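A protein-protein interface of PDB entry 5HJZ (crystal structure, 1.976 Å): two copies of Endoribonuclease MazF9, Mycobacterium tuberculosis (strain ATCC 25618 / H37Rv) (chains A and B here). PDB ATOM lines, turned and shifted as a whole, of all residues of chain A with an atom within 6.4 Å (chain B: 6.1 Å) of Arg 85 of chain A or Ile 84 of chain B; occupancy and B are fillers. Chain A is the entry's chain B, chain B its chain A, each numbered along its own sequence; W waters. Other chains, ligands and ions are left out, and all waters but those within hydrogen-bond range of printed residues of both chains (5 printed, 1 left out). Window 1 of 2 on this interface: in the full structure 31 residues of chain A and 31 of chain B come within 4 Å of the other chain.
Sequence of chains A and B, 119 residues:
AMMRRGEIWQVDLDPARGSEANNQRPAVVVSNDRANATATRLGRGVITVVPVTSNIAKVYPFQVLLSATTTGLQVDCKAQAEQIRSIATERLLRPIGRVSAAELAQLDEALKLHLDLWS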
ATOM      1  N   ASP A  12     -25.696  -2.204   0.174  1.00  0.00           N
ATOM      2  CA  ASP A  12     -24.889  -1.565  -0.857  1.00  0.00           C
ATOM      3  C   ASP A  12     -23.439  -2.036  -0.761  1.00  0.00           C
ATOM      4  O   ASP A  12     -22.732  -1.694   0.184  1.00  0.00           O
ATOM      5  CB  ASP A  12     -24.977  -0.043  -0.724  1.00  0.00           C
ATOM      6  CG  ASP A  12     -24.151   0.690  -1.761  1.00  0.00           C
ATOM      7  OD1 ASP A  12     -23.859   0.107  -2.827  1.00  0.00           O
ATOM      8  OD2 ASP A  12     -23.802   1.863  -1.510  1.00  0.00           O
ATOM      9  N   LEU A  13     -23.002  -2.818  -1.744  1.00  0.00           N
ATOM     10  CA  LEU A  13     -21.675  -3.431  -1.705  1.00  0.00           C
ATOM     11  C   LEU A  13     -20.658  -2.717  -2.593  1.00  0.00           C
ATOM     12  O   LEU A  13     -19.482  -3.084  -2.620  1.00  0.00           O
ATOM     13  CB  LEU A  13     -21.767  -4.903  -2.111  1.00  0.00           C
ATOM     14  CG  LEU A  13     -22.588  -5.793  -1.175  1.00  0.00           C
ATOM     15  CD1 LEU A  13     -22.630  -7.227  -1.681  1.00  0.00           C
ATOM     16  CD2 LEU A  13     -22.028  -5.735   0.240  1.00  0.00           C
ATOM     17  N   ASP A  14     -21.110  -1.697  -3.317  1.00  0.00           N
ATOM     18  CA  ASP A  14     -20.235  -0.947  -4.213  1.00  0.00           C
ATOM     19  C   ASP A  14     -19.373   0.058  -3.451  1.00  0.00           C
ATOM     20  O   ASP A  14     -19.775   0.546  -2.395  1.00  0.00           O
ATOM     21  CB  ASP A  14     -21.065  -0.231  -5.284  1.00  0.00           C
ATOM     22  CG  ASP A  14     -21.529  -1.168  -6.382  1.00  0.00           C
ATOM     23  OD1 ASP A  14     -20.893  -2.226  -6.568  1.00  0.00           O
ATOM     24  OD2 ASP A  14     -22.526  -0.844  -7.059  1.00  0.00           O
ATOM     25  N   PRO A  15     -18.172   0.360  -3.977  1.00  0.00           N
ATOM     26  CA  PRO A  15     -17.589  -0.271  -5.164  1.00  0.00           C
ATOM     27  C   PRO A  15     -16.850  -1.559  -4.815  1.00  0.00           C
ATOM     28  O   PRO A  15     -16.271  -1.657  -3.734  1.00  0.00           O
ATOM     29  CB  PRO A  15     -16.625   0.794  -5.683  1.00  0.00           C
ATOM     30  CG  PRO A  15     -16.174   1.494  -4.451  1.00  0.00           C
ATOM     31  CD  PRO A  15     -17.340   1.475  -3.489  1.00  0.00           C
ATOM     32  N   GLU A  20     -15.200  -9.902  -5.787  1.00  0.00           N
ATOM     33  CA  GLU A  20     -16.009  -9.460  -4.658  1.00  0.00           C
ATOM     34  C   GLU A  20     -17.452  -9.241  -5.095  1.00  0.00           C
ATOM     35  O   GLU A  20     -17.705  -8.711  -6.178  1.00  0.00           O
ATOM     36  CB  GLU A  20     -15.441  -8.175  -4.051  1.00  0.00           C
ATOM     37  CG  GLU A  20     -14.080  -8.334  -3.391  1.00  0.00           C
ATOM     38  CD  GLU A  20     -13.400  -7.001  -3.145  1.00  0.00           C
ATOM     39  OE1 GLU A  20     -14.042  -5.955  -3.375  1.00  0.00           O
ATOM     40  OE2 GLU A  20     -12.223  -6.996  -2.729  1.00  0.00           O
ATOM     41  N   ALA A  21     -18.394  -9.661  -4.256  1.00  0.00           N
ATOM     42  CA  ALA A  21     -19.808  -9.414  -4.513  1.00  0.00           C
ATOM     43  C   ALA A  21     -20.054  -7.912  -4.616  1.00  0.00           C
ATOM     44  O   ALA A  21     -19.514  -7.135  -3.826  1.00  0.00           O
ATOM     45  CB  ALA A  21     -20.668 -10.031  -3.420  1.00  0.00           C
ATOM     46  N   ILE A  47     -21.848  -4.004  11.025  1.00  0.00           N
ATOM     47  CA  ILE A  47     -22.501  -5.287  11.245  1.00  0.00           C
ATOM     48  C   ILE A  47     -22.040  -6.218  10.130  1.00  0.00           C
ATOM     49  O   ILE A  47     -21.518  -5.758   9.115  1.00  0.00           O
ATOM     50  CB  ILE A  47     -24.037  -5.172  11.263  1.00  0.00           C
ATOM     51  CG1 ILE A  47     -24.553  -4.669   9.917  1.00  0.00           C
ATOM     52  CG2 ILE A  47     -24.498  -4.254  12.390  1.00  0.00           C
ATOM     53  CD1 ILE A  47     -25.443  -5.659   9.212  1.00  0.00           C
ATOM     54  N   THR A  48     -22.218  -7.520  10.311  1.00  0.00           N
ATOM     55  CA  THR A  48     -21.670  -8.479   9.357  1.00  0.00           C
ATOM     56  C   THR A  48     -22.763  -9.205   8.578  1.00  0.00           C
ATOM     57  O   THR A  48     -23.723  -9.710   9.157  1.00  0.00           O
ATOM     58  CB  THR A  48     -20.774  -9.513  10.063  1.00  0.00           C
ATOM     59  OG1 THR A  48     -19.752  -8.833  10.803  1.00  0.00           O
ATOM     60  CG2 THR A  48     -20.119 -10.432   9.048  1.00  0.00           C
ATOM     61  N   VAL A  49     -22.605  -9.252   7.259  1.00  0.00           N
ATOM     62  CA  VAL A  49     -23.592  -9.886   6.396  1.00  0.00           C
ATOM     63  C   VAL A  49     -22.977 -10.910   5.448  1.00  0.00           C
ATOM     64  O   VAL A  49     -21.772 -10.902   5.191  1.00  0.00           O
ATOM     65  CB  VAL A  49     -24.353  -8.847   5.552  1.00  0.00           C
ATOM     66  CG1 VAL A  49     -25.164  -7.931   6.446  1.00  0.00           C
ATOM     67  CG2 VAL A  49     -23.385  -8.047   4.694  1.00  0.00           C
ATOM     68  N   VAL A  50     -23.829 -11.794   4.939  1.00  0.00           N
ATOM     69  CA  VAL A  50     -23.446 -12.755   3.915  1.00  0.00           C
ATOM     70  C   VAL A  50     -24.247 -12.477   2.646  1.00  0.00           C
ATOM     71  O   VAL A  50     -25.469 -12.634   2.634  1.00  0.00           O
ATOM     72  CB  VAL A  50     -23.676 -14.205   4.383  1.00  0.00           C
ATOM     73  CG1 VAL A  50     -23.626 -15.166   3.207  1.00  0.00           C
ATOM     74  CG2 VAL A  50     -22.652 -14.590   5.443  1.00  0.00           C
ATOM     75  N   PRO A  51     -23.558 -12.042   1.579  1.00  0.00           N
ATOM     76  CA  PRO A  51     -24.185 -11.688   0.300  1.00  0.00           C
ATOM     77  C   PRO A  51     -24.973 -12.839  -0.316  1.00  0.00           C
ATOM     78  O   PRO A  51     -24.727 -14.007  -0.012  1.00  0.00           O
ATOM     79  CB  PRO A  51     -22.992 -11.317  -0.586  1.00  0.00           C
ATOM     80  CG  PRO A  51     -21.930 -10.909   0.366  1.00  0.00           C
ATOM     81  CD  PRO A  51     -22.108 -11.791   1.563  1.00  0.00           C
ATOM     82  N   ALA A  81     -21.295 -17.731   1.993  1.00  0.00           N
ATOM     83  CA  ALA A  81     -20.522 -17.511   3.209  1.00  0.00           C
ATOM     84  C   ALA A  81     -19.083 -17.127   2.884  1.00  0.00           C
ATOM     85  O   ALA A  81     -18.422 -16.462   3.678  1.00  0.00           O
ATOM     86  CB  ALA A  81     -20.556 -18.746   4.095  1.00  0.00           C
ATOM     87  N   GLN A  83     -18.281 -15.058   0.765  1.00  0.00           N
ATOM     88  CA  GLN A  83     -18.310 -13.641   0.411  1.00  0.00           C
ATOM     89  C   GLN A  83     -18.625 -12.765   1.621  1.00  0.00           C
ATOM     90  O   GLN A  83     -18.941 -11.584   1.473  1.00  0.00           O
ATOM     91  CB  GLN A  83     -19.338 -13.388  -0.695  1.00  0.00           C
ATOM     92  CG  GLN A  83     -18.939 -13.926  -2.063  1.00  0.00           C
ATOM     93  CD  GLN A  83     -17.987 -13.004  -2.802  1.00  0.00           C
ATOM     94  OE1 GLN A  83     -17.773 -11.860  -2.399  1.00  0.00           O
ATOM     95  NE2 GLN A  83     -17.412 -13.496  -3.894  1.00  0.00           N
ATOM     96  N   ILE A  84     -18.532 -13.348   2.813  1.00  0.00           N
ATOM     97  CA  ILE A  84     -18.881 -12.653   4.049  1.00  0.00           C
ATOM     98  C   ILE A  84     -18.076 -11.365   4.243  1.00  0.00           C
ATOM     99  O   ILE A  84     -16.860 -11.342   4.056  1.00  0.00           O
ATOM    100  CB  ILE A  84     -18.679 -13.577   5.281  1.00  0.00           C
ATOM    101  CG1 ILE A  84     -19.098 -12.866   6.568  1.00  0.00           C
ATOM    102  CG2 ILE A  84     -17.230 -14.063   5.379  1.00  0.00           C
ATOM    103  CD1 ILE A  84     -19.012 -13.732   7.801  1.00  0.00           C
ATOM    104  N   ARG A  85     -18.758 -10.281   4.597  1.00  0.00           N
ATOM    105  CA  ARG A  85     -18.051  -9.047   4.919  1.00  0.00           C
ATOM    106  C   ARG A  85     -18.822  -8.186   5.911  1.00  0.00           C
ATOM    107  O   ARG A  85     -20.055  -8.134   5.894  1.00  0.00           O
ATOM    108  CB  ARG A  85     -17.752  -8.239   3.650  1.00  0.00           C
ATOM    109  CG  ARG A  85     -18.942  -7.507   3.051  1.00  0.00           C
ATOM    110  CD  ARG A  85     -18.484  -6.315   2.222  1.00  0.00           C
ATOM    111  NE  ARG A  85     -17.636  -5.413   3.000  1.00  0.00           N
ATOM    112  CZ  ARG A  85     -17.181  -4.246   2.558  1.00  0.00           C
ATOM    113  NH1 ARG A  85     -17.494  -3.827   1.339  1.00  0.00           N
ATOM    114  NH2 ARG A  85     -16.414  -3.492   3.337  1.00  0.00           N
ATOM    115  N   SER A  86     -18.078  -7.523   6.788  1.00  0.00           N
ATOM    116  CA  SER A  86     -18.661  -6.544   7.689  1.00  0.00           C
ATOM    117  C   SER A  86     -18.911  -5.259   6.916  1.00  0.00           C
ATOM    118  O   SER A  86     -18.096  -4.855   6.086  1.00  0.00           O
ATOM    119  CB  SER A  86     -17.746  -6.284   8.886  1.00  0.00           C
ATOM    120  OG  SER A  86     -16.501  -5.747   8.470  1.00  0.00           O
ATOM    121  N   ILE A  87     -20.047  -4.625   7.180  1.00  0.00           N
ATOM    122  CA  ILE A  87     -20.397  -3.388   6.500  1.00  0.00           C
ATOM    123  C   ILE A  87     -20.875  -2.337   7.493  1.00  0.00           C
ATOM    124  O   ILE A  87     -21.498  -2.661   8.503  1.00  0.00           O
ATOM    125  CB  ILE A  87     -21.492  -3.616   5.435  1.00  0.00           C
ATOM    126  CG1 ILE A  87     -22.717  -4.287   6.057  1.00  0.00           C
ATOM    127  CG2 ILE A  87     -20.958  -4.458   4.285  1.00  0.00           C
ATOM    128  CD1 ILE A  87     -23.892  -4.418   5.105  1.00  0.00           C
ATOM    129  N   ALA A  88     -20.567  -1.076   7.206  1.00  0.00           N
ATOM    130  CA  ALA A  88     -21.105   0.030   7.986  1.00  0.00           C
ATOM    131  C   ALA A  88     -22.622   0.034   7.872  1.00  0.00           C
ATOM    132  O   ALA A  88     -23.170  -0.378   6.852  1.00  0.00           O
ATOM    133  CB  ALA A  88     -20.529   1.352   7.513  1.00  0.00           C
ATOM    134  N   ARG A  91     -24.631   1.251   4.853  1.00  0.00           N
ATOM    135  CA  ARG A  91     -24.759   0.414   3.664  1.00  0.00           C
ATOM    136  C   ARG A  91     -26.074  -0.359   3.677  1.00  0.00           C
ATOM    137  O   ARG A  91     -26.470  -0.945   2.671  1.00  0.00           O
ATOM    138  CB  ARG A  91     -23.585  -0.562   3.552  1.00  0.00           C
ATOM    139  CG  ARG A  91     -22.265   0.065   3.138  1.00  0.00           C
ATOM    140  CD  ARG A  91     -21.226  -1.022   2.881  1.00  0.00           C
ATOM    141  NE  ARG A  91     -19.902  -0.488   2.578  1.00  0.00           N
ATOM    142  CZ  ARG A  91     -19.381  -0.417   1.356  1.00  0.00           C
ATOM    143  NH1 ARG A  91     -20.072  -0.845   0.308  1.00  0.00           N
ATOM    144  NH2 ARG A  91     -18.165   0.082   1.182  1.00  0.00           N
ATOM    145  N   LEU A 115     -14.611 -20.675   7.473  1.00  0.00           N
ATOM    146  CA  LEU A 115     -13.652 -19.995   8.336  1.00  0.00           C
ATOM    147  C   LEU A 115     -12.855 -20.955   9.213  1.00  0.00           C
ATOM    148  O   LEU A 115     -12.140 -20.524  10.117  1.00  0.00           O
ATOM    149  CB  LEU A 115     -14.376 -18.971   9.211  1.00  0.00           C
ATOM    150  CG  LEU A 115     -15.017 -17.817   8.439  1.00  0.00           C
ATOM    151  CD1 LEU A 115     -15.960 -17.029   9.327  1.00  0.00           C
ATOM    152  CD2 LEU A 115     -13.946 -16.907   7.856  1.00  0.00           C
ATOM    153  N   PRO B  15     -11.888   2.014  -1.060  1.00  0.00           N
ATOM    154  CA  PRO B  15     -12.503   2.990  -0.154  1.00  0.00           C
ATOM    155  C   PRO B  15     -13.379   2.329   0.905  1.00  0.00           C
ATOM    156  O   PRO B  15     -14.027   1.320   0.629  1.00  0.00           O
ATOM    157  CB  PRO B  15     -13.343   3.854  -1.096  1.00  0.00           C
ATOM    158  CG  PRO B  15     -13.742   2.920  -2.177  1.00  0.00           C
ATOM    159  CD  PRO B  15     -12.582   1.966  -2.360  1.00  0.00           C
ATOM    160  N   GLU B  20     -15.903   1.153   8.741  1.00  0.00           N
ATOM    161  CA  GLU B  20     -15.124   0.095   8.107  1.00  0.00           C
ATOM    162  C   GLU B  20     -13.646   0.474   8.128  1.00  0.00           C
ATOM    163  O   GLU B  20     -13.293   1.616   7.832  1.00  0.00           O
ATOM    164  CB  GLU B  20     -15.599  -0.146   6.669  1.00  0.00           C
ATOM    165  CG  GLU B  20     -17.022  -0.680   6.569  1.00  0.00           C
ATOM    166  CD  GLU B  20     -17.648  -0.449   5.203  1.00  0.00           C
ATOM    167  OE1 GLU B  20     -16.951   0.049   4.294  1.00  0.00           O
ATOM    168  OE2 GLU B  20     -18.844  -0.763   5.042  1.00  0.00           O
ATOM    169  N   VAL B  30      -8.154 -15.597   7.493  1.00  0.00           N
ATOM    170  CA  VAL B  30      -8.960 -16.490   8.322  1.00  0.00           C
ATOM    171  C   VAL B  30      -9.809 -17.464   7.506  1.00  0.00           C
ATOM    172  O   VAL B  30     -10.413 -18.382   8.061  1.00  0.00           O
ATOM    173  CB  VAL B  30      -9.889 -15.698   9.263  1.00  0.00           C
ATOM    174  CG1 VAL B  30      -9.069 -14.889  10.256  1.00  0.00           C
ATOM    175  CG2 VAL B  30     -10.813 -14.798   8.461  1.00  0.00           C
ATOM    176  N   THR B  48     -10.779 -14.364   2.951  1.00  0.00           N
ATOM    177  CA  THR B  48     -11.371 -13.637   4.065  1.00  0.00           C
ATOM    178  C   THR B  48     -10.310 -13.261   5.091  1.00  0.00           C
ATOM    179  O   THR B  48      -9.527 -14.104   5.524  1.00  0.00           O
ATOM    180  CB  THR B  48     -12.480 -14.460   4.738  1.00  0.00           C
ATOM    181  OG1 THR B  48     -13.450 -14.841   3.757  1.00  0.00           O
ATOM    182  CG2 THR B  48     -13.163 -13.644   5.816  1.00  0.00           C
ATOM    183  N   VAL B  49     -10.282 -11.985   5.467  1.00  0.00           N
ATOM    184  CA  VAL B  49      -9.262 -11.486   6.382  1.00  0.00           C
ATOM    185  C   VAL B  49      -9.850 -10.723   7.562  1.00  0.00           C
ATOM    186  O   VAL B  49     -10.998 -10.276   7.525  1.00  0.00           O
ATOM    187  CB  VAL B  49      -8.255 -10.563   5.663  1.00  0.00           C
ATOM    188  CG1 VAL B  49      -7.557 -11.305   4.534  1.00  0.00           C
ATOM    189  CG2 VAL B  49      -8.953  -9.314   5.142  1.00  0.00           C
ATOM    190  N   VAL B  50      -9.046 -10.585   8.611  1.00  0.00           N
ATOM    191  CA  VAL B  50      -9.415  -9.797   9.780  1.00  0.00           C
ATOM    192  C   VAL B  50      -8.463  -8.616   9.926  1.00  0.00           C
ATOM    193  O   VAL B  50      -7.289  -8.794  10.256  1.00  0.00           O
ATOM    194  CB  VAL B  50      -9.399 -10.644  11.068  1.00  0.00           C
ATOM    195  CG1 VAL B  50      -9.467  -9.752  12.301  1.00  0.00           C
ATOM    196  CG2 VAL B  50     -10.551 -11.636  11.060  1.00  0.00           C
ATOM    197  N   PRO B  51      -8.968  -7.404   9.659  1.00  0.00           N
ATOM    198  CA  PRO B  51      -8.189  -6.167   9.749  1.00  0.00           C
ATOM    199  C   PRO B  51      -7.596  -5.953  11.135  1.00  0.00           C
ATOM    200  O   PRO B  51      -8.117  -6.452  12.133  1.00  0.00           O
ATOM    201  CB  PRO B  51      -9.217  -5.080   9.420  1.00  0.00           C
ATOM    202  CG  PRO B  51     -10.220  -5.772   8.572  1.00  0.00           C
ATOM    203  CD  PRO B  51     -10.325  -7.156   9.146  1.00  0.00           C
ATOM    204  N   GLN B  80      -9.407  -7.218  14.702  1.00  0.00           N
ATOM    205  CA  GLN B  80     -10.825  -6.927  14.886  1.00  0.00           C
ATOM    206  C   GLN B  80     -11.701  -7.921  14.133  1.00  0.00           C
ATOM    207  O   GLN B  80     -11.951  -7.758  12.939  1.00  0.00           O
ATOM    208  CB  GLN B  80     -11.135  -5.503  14.425  1.00  0.00           C
ATOM    209  CG  GLN B  80     -10.394  -4.428  15.199  1.00  0.00           C
ATOM    210  CD  GLN B  80     -10.523  -3.057  14.565  1.00  0.00           C
ATOM    211  OE1 GLN B  80     -10.107  -2.846  13.424  1.00  0.00           O
ATOM    212  NE2 GLN B  80     -11.102  -2.117  15.301  1.00  0.00           N
ATOM    213  N   ALA B  81     -12.166  -8.950  14.834  1.00  0.00           N
ATOM    214  CA  ALA B  81     -12.984  -9.987  14.212  1.00  0.00           C
ATOM    215  C   ALA B  81     -14.304  -9.424  13.693  1.00  0.00           C
ATOM    216  O   ALA B  81     -14.892  -9.971  12.763  1.00  0.00           O
ATOM    217  CB  ALA B  81     -13.240 -11.121  15.191  1.00  0.00           C
ATOM    218  N   GLU B  82     -14.761  -8.324  14.288  1.00  0.00           N
ATOM    219  CA  GLU B  82     -16.004  -7.690  13.858  1.00  0.00           C
ATOM    220  C   GLU B  82     -15.798  -6.921  12.555  1.00  0.00           C
ATOM    221  O   GLU B  82     -16.760  -6.469  11.934  1.00  0.00           O
ATOM    222  CB  GLU B  82     -16.544  -6.753  14.945  1.00  0.00           C
ATOM    223  CG  GLU B  82     -15.893  -5.373  14.980  1.00  0.00           C
ATOM    224  CD  GLU B  82     -14.554  -5.354  15.699  1.00  0.00           C
ATOM    225  OE1 GLU B  82     -13.980  -6.438  15.941  1.00  0.00           O
ATOM    226  OE2 GLU B  82     -14.078  -4.247  16.025  1.00  0.00           O
ATOM    227  N   GLN B  83     -14.538  -6.775  12.152  1.00  0.00           N
ATOM    228  CA  GLN B  83     -14.192  -6.096  10.907  1.00  0.00           C
ATOM    229  C   GLN B  83     -13.925  -7.093   9.783  1.00  0.00           C
ATOM    230  O   GLN B  83     -13.401  -6.723   8.731  1.00  0.00           O
ATOM    231  CB  GLN B  83     -12.966  -5.198  11.105  1.00  0.00           C
ATOM    232  CG  GLN B  83     -13.234  -3.929  11.902  1.00  0.00           C
ATOM    233  CD  GLN B  83     -13.961  -2.868  11.094  1.00  0.00           C
ATOM    234  OE1 GLN B  83     -13.824  -2.798   9.872  1.00  0.00           O
ATOM    235  NE2 GLN B  83     -14.738  -2.038  11.777  1.00  0.00           N
ATOM    236  N   ILE B  84     -14.293  -8.352  10.017  1.00  0.00           N
ATOM    237  CA  ILE B  84     -14.082  -9.432   9.054  1.00  0.00           C
ATOM    238  C   ILE B  84     -14.565  -9.047   7.653  1.00  0.00           C
ATOM    239  O   ILE B  84     -15.636  -8.458   7.490  1.00  0.00           O
ATOM    240  CB  ILE B  84     -14.787 -10.731   9.516  1.00  0.00           C
ATOM    241  CG1 ILE B  84     -14.489 -11.880   8.553  1.00  0.00           C
ATOM    242  CG2 ILE B  84     -16.297 -10.514   9.679  1.00  0.00           C
ATOM    243  CD1 ILE B  84     -15.070 -13.214   8.983  1.00  0.00           C
ATOM    244  N   ARG B  85     -13.757  -9.353   6.644  1.00  0.00           N
ATOM    245  CA  ARG B  85     -14.062  -8.924   5.283  1.00  0.00           C
ATOM    246  C   ARG B  85     -13.465  -9.850   4.230  1.00  0.00           C
ATOM    247  O   ARG B  85     -12.266 -10.133   4.248  1.00  0.00           O
ATOM    248  CB  ARG B  85     -13.557  -7.495   5.059  1.00  0.00           C
ATOM    249  CG  ARG B  85     -13.891  -6.921   3.687  1.00  0.00           C
ATOM    250  CD  ARG B  85     -13.356  -5.504   3.530  1.00  0.00           C
ATOM    251  NE  ARG B  85     -13.662  -4.942   2.217  1.00  0.00           N
ATOM    252  CZ  ARG B  85     -13.283  -3.733   1.813  1.00  0.00           C
ATOM    253  NH1 ARG B  85     -12.576  -2.952   2.620  1.00  0.00           N
ATOM    254  NH2 ARG B  85     -13.609  -3.305   0.601  1.00  0.00           N
ATOM    255  N   SER B  86     -14.307 -10.320   3.314  1.00  0.00           N
ATOM    256  CA  SER B  86     -13.834 -11.098   2.176  1.00  0.00           C
ATOM    257  C   SER B  86     -13.399 -10.157   1.061  1.00  0.00           C
ATOM    258  O   SER B  86     -14.178  -9.318   0.605  1.00  0.00           O
ATOM    259  CB  SER B  86     -14.916 -12.056   1.674  1.00  0.00           C
ATOM    260  OG  SER B  86     -15.289 -12.973   2.687  1.00  0.00           O
ATOM    261  N   LEU B 111     -13.917 -14.918  16.529  1.00  0.00           N
ATOM    262  CA  LEU B 111     -14.794 -15.069  15.372  1.00  0.00           C
ATOM    263  C   LEU B 111     -16.084 -15.799  15.738  1.00  0.00           C
ATOM    264  O   LEU B 111     -17.169 -15.408  15.307  1.00  0.00           O
ATOM    265  CB  LEU B 111     -14.073 -15.811  14.245  1.00  0.00           C
ATOM    266  CG  LEU B 111     -13.032 -15.014  13.457  1.00  0.00           C
ATOM    267  CD1 LEU B 111     -12.192 -15.937  12.581  1.00  0.00           C
ATOM    268  CD2 LEU B 111     -13.711 -13.945  12.613  1.00  0.00           C
ATOM    269  N   HIS B 114     -18.203 -13.319  17.720  1.00  0.00           N
ATOM    270  CA  HIS B 114     -18.786 -12.276  16.890  1.00  0.00           C
ATOM    271  C   HIS B 114     -19.916 -12.800  16.006  1.00  0.00           C
ATOM    272  O   HIS B 114     -20.959 -12.160  15.878  1.00  0.00           O
ATOM    273  CB  HIS B 114     -17.718 -11.621  16.016  1.00  0.00           C
ATOM    274  CG  HIS B 114     -18.273 -10.629  15.044  1.00  0.00           C
ATOM    275  ND1 HIS B 114     -18.898  -9.466  15.445  1.00  0.00           N
ATOM    276  CD2 HIS B 114     -18.319 -10.632  13.691  1.00  0.00           C
ATOM    277  CE1 HIS B 114     -19.294  -8.793  14.380  1.00  0.00           C
ATOM    278  NE2 HIS B 114     -18.955  -9.478  13.302  1.00  0.00           N
ATOM    279  N   LEU B 115     -19.707 -13.965  15.401  1.00  0.00           N
ATOM    280  CA  LEU B 115     -20.676 -14.514  14.456  1.00  0.00           C
ATOM    281  C   LEU B 115     -21.714 -15.410  15.128  1.00  0.00           C
ATOM    282  O   LEU B 115     -22.517 -16.052  14.447  1.00  0.00           O
ATOM    283  CB  LEU B 115     -19.954 -15.294  13.357  1.00  0.00           C
ATOM    284  CG  LEU B 115     -18.967 -14.477  12.523  1.00  0.00           C
ATOM    285  CD1 LEU B 115     -18.249 -15.373  11.533  1.00  0.00           C
ATOM    286  CD2 LEU B 115     -19.682 -13.341  11.806  1.00  0.00           C
HETATM  287  O   HOH W   1     -16.389  -9.387  -1.345  1.00  0.00           O
HETATM  288  O   HOH W   2     -19.569  -6.429  12.237  1.00  0.00           O
HETATM  289  O   HOH W   3     -13.522  -4.249   7.628  1.00  0.00           O
HETATM  290  O   HOH W   4     -15.399  -4.891  -1.409  1.00  0.00           O
HETATM  291  O   HOH W   5     -15.280  -6.642   0.757  1.00  0.00           O
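Arg 85 of chain A touches just these residues of chain B: Glu 20 (3.7 Å), Ile 84 (3.6 Å) and Arg 85 (3.3 Å). Ile 84 of chain B touches four residues of chain A. Of the printed residues of chain A, Arg 85 of chain B touches Ile 84 and Arg 85. Of the printed residues of chain B, Ala 88 of chain A touches Glu 20 (2.8 Å). Val 49 of chain B touches none of the printed residues of chain A. The nearest residue of chain A that does not touch Ile 84 of chain B is Ile 84 of chain A (4.1 Å). The nearest printed residue of chain B that does not touch Gln 83 of chain A is Thr 48 of chain B (5.7 Å).
Among the printed residues, pairs that only touch across the chains: Ser 86 of chain A with Glu 82 of chain B (3.2 Å), Ile 87 of chain A with Glu 20 of chain B (3.4 Å), Gln 83 of chain A with Ser 86 of chain B (3.5 Å), Arg 85 of chain A with Ile 84 of chain B (3.6 Å), Leu 115 of chain A with Leu 115 of chain B (3.6 Å), Pro 15 of chain A with Pro 15 of chain B (3.6 Å), Ile 84 of chain A with Arg 85 of chain B (3.7 Å), Thr 48 of chain A with Ile 84 of chain B (3.9 Å), Leu 115 of chain A with Thr 48 of chain B (3.9 Å), Leu 115 of chain A with Ile 84 of chain B (3.9 Å) and Thr 48 of chain A with Glu 82 of chain B (3.98 Å).
Hydrophobic or aromatic side chains of chain B within 4 Å of the printed part of chain A: Pro 15, Val 30, Ile 84, His 114 and Leu 115. Of the 20 printed residues of chain A, 10 touch a printed residue of chain B. Hydrophobic or aromatic side chains of chain A within 4 Å of the printed part of chain B: Pro 15, Ile 84, Ile 87, Ala 88 and Leu 115. Among the printed residues, 20 pairs touch across the chains. Among the printed residues, Asp or Glu carboxylates within 4 Å of a Lys or Arg side-chain nitrogen of the other chain: Arg 85 of chain A with Glu 20 of chain B (3.7 Å) and Arg 91 of chain A with Glu 20 of chain B (2.7 Å).
Water W3 lies within hydrogen-bond range of OE1 of Gln 83 of chain B (2.7 Å) and OG of Ser 86 of chain A (3.4 Å). Water W5 lies within hydrogen-bond range of the guanidinium group (NE) of Arg 85 of chain B, the backbone carbonyl oxygen (O) of Ser 86 of chain B and the guanidinium group (NE) of Arg 85 of chain A.
The backbone carbonyl oxygen (O) of Asp 12 of chain A is in hydrogen-bond range of the guanidinium group (NH1) of Arg 91 of chain A, 2.8 Å away. NH1 of Arg 91 of chain A is in hydrogen-bond range of O of Asp 14 of chain A. The backbone NH (N) of Ile 87 of chain A sits at hydrogen-bond distance from the backbone carbonyl oxygen (O) of Ile 47 of chain A. O of Arg 85 of chain A lies within hydrogen-bond range of N of Val 49 of chain A, 3.1 Å away.
Thr 48 of chain A touches Ile 84 of chain B, but with the chains exchanged Ile 84 of chain A does not touch Thr 48 of chain B (4.1 Å). Arg 85 of chain A touches Glu 20 of chain B, but with the chains exchanged Glu 20 of chain A does not touch Arg 85 of chain B (4.8 Å). Leu 115 of chain A touches Ile 84 of chain B, but with the chains exchanged Ile 84 of chain A does not touch Leu 115 of chain B (4.1 Å).
The side-chain carboxylate of Glu 20 of chain B is in salt-bridge range of the guanidinium group of Arg 85 of chain A. OE2 of Glu 20 of chain B lies within hydrogen-bond range of N of Ala 88 of chain A, 2.8 Å away. The side-chain carboxylate of Glu 20 of chain B is in salt-bridge range of the guanidinium group of Arg 91 of chain A. The backbone carbonyl oxygen (O) of Gln 83 of chain B sits close to the side-chain hydroxyl (OG) of Ser 86 of chain A, at 3.3 Å. N of Ser 86 of chain A lies within hydrogen-bond range of O of Ile 84 of chain B (2.7 Å). The side-chain hydroxyl (OG) of Ser 86 of chain B is in hydrogen-bond range of the backbone carbonyl oxygen (O) of Ile 84 of chain A (2.6 Å). A ring nitrogen (NE2) of His 114 of chain B is in hydrogen-bond range of the side-chain hydroxyl (OG1) of Thr 48 of chain A (2.7 Å). NE of Arg 85 of chain B sits close to NH2 of Arg 85 of chain A (3.3 Å). The backbone carbonyl oxygen (O) of Val 30 of chain B lies close to the backbone carbonyl oxygen (O) of Leu 115 of chain A, at 3.4 Å.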
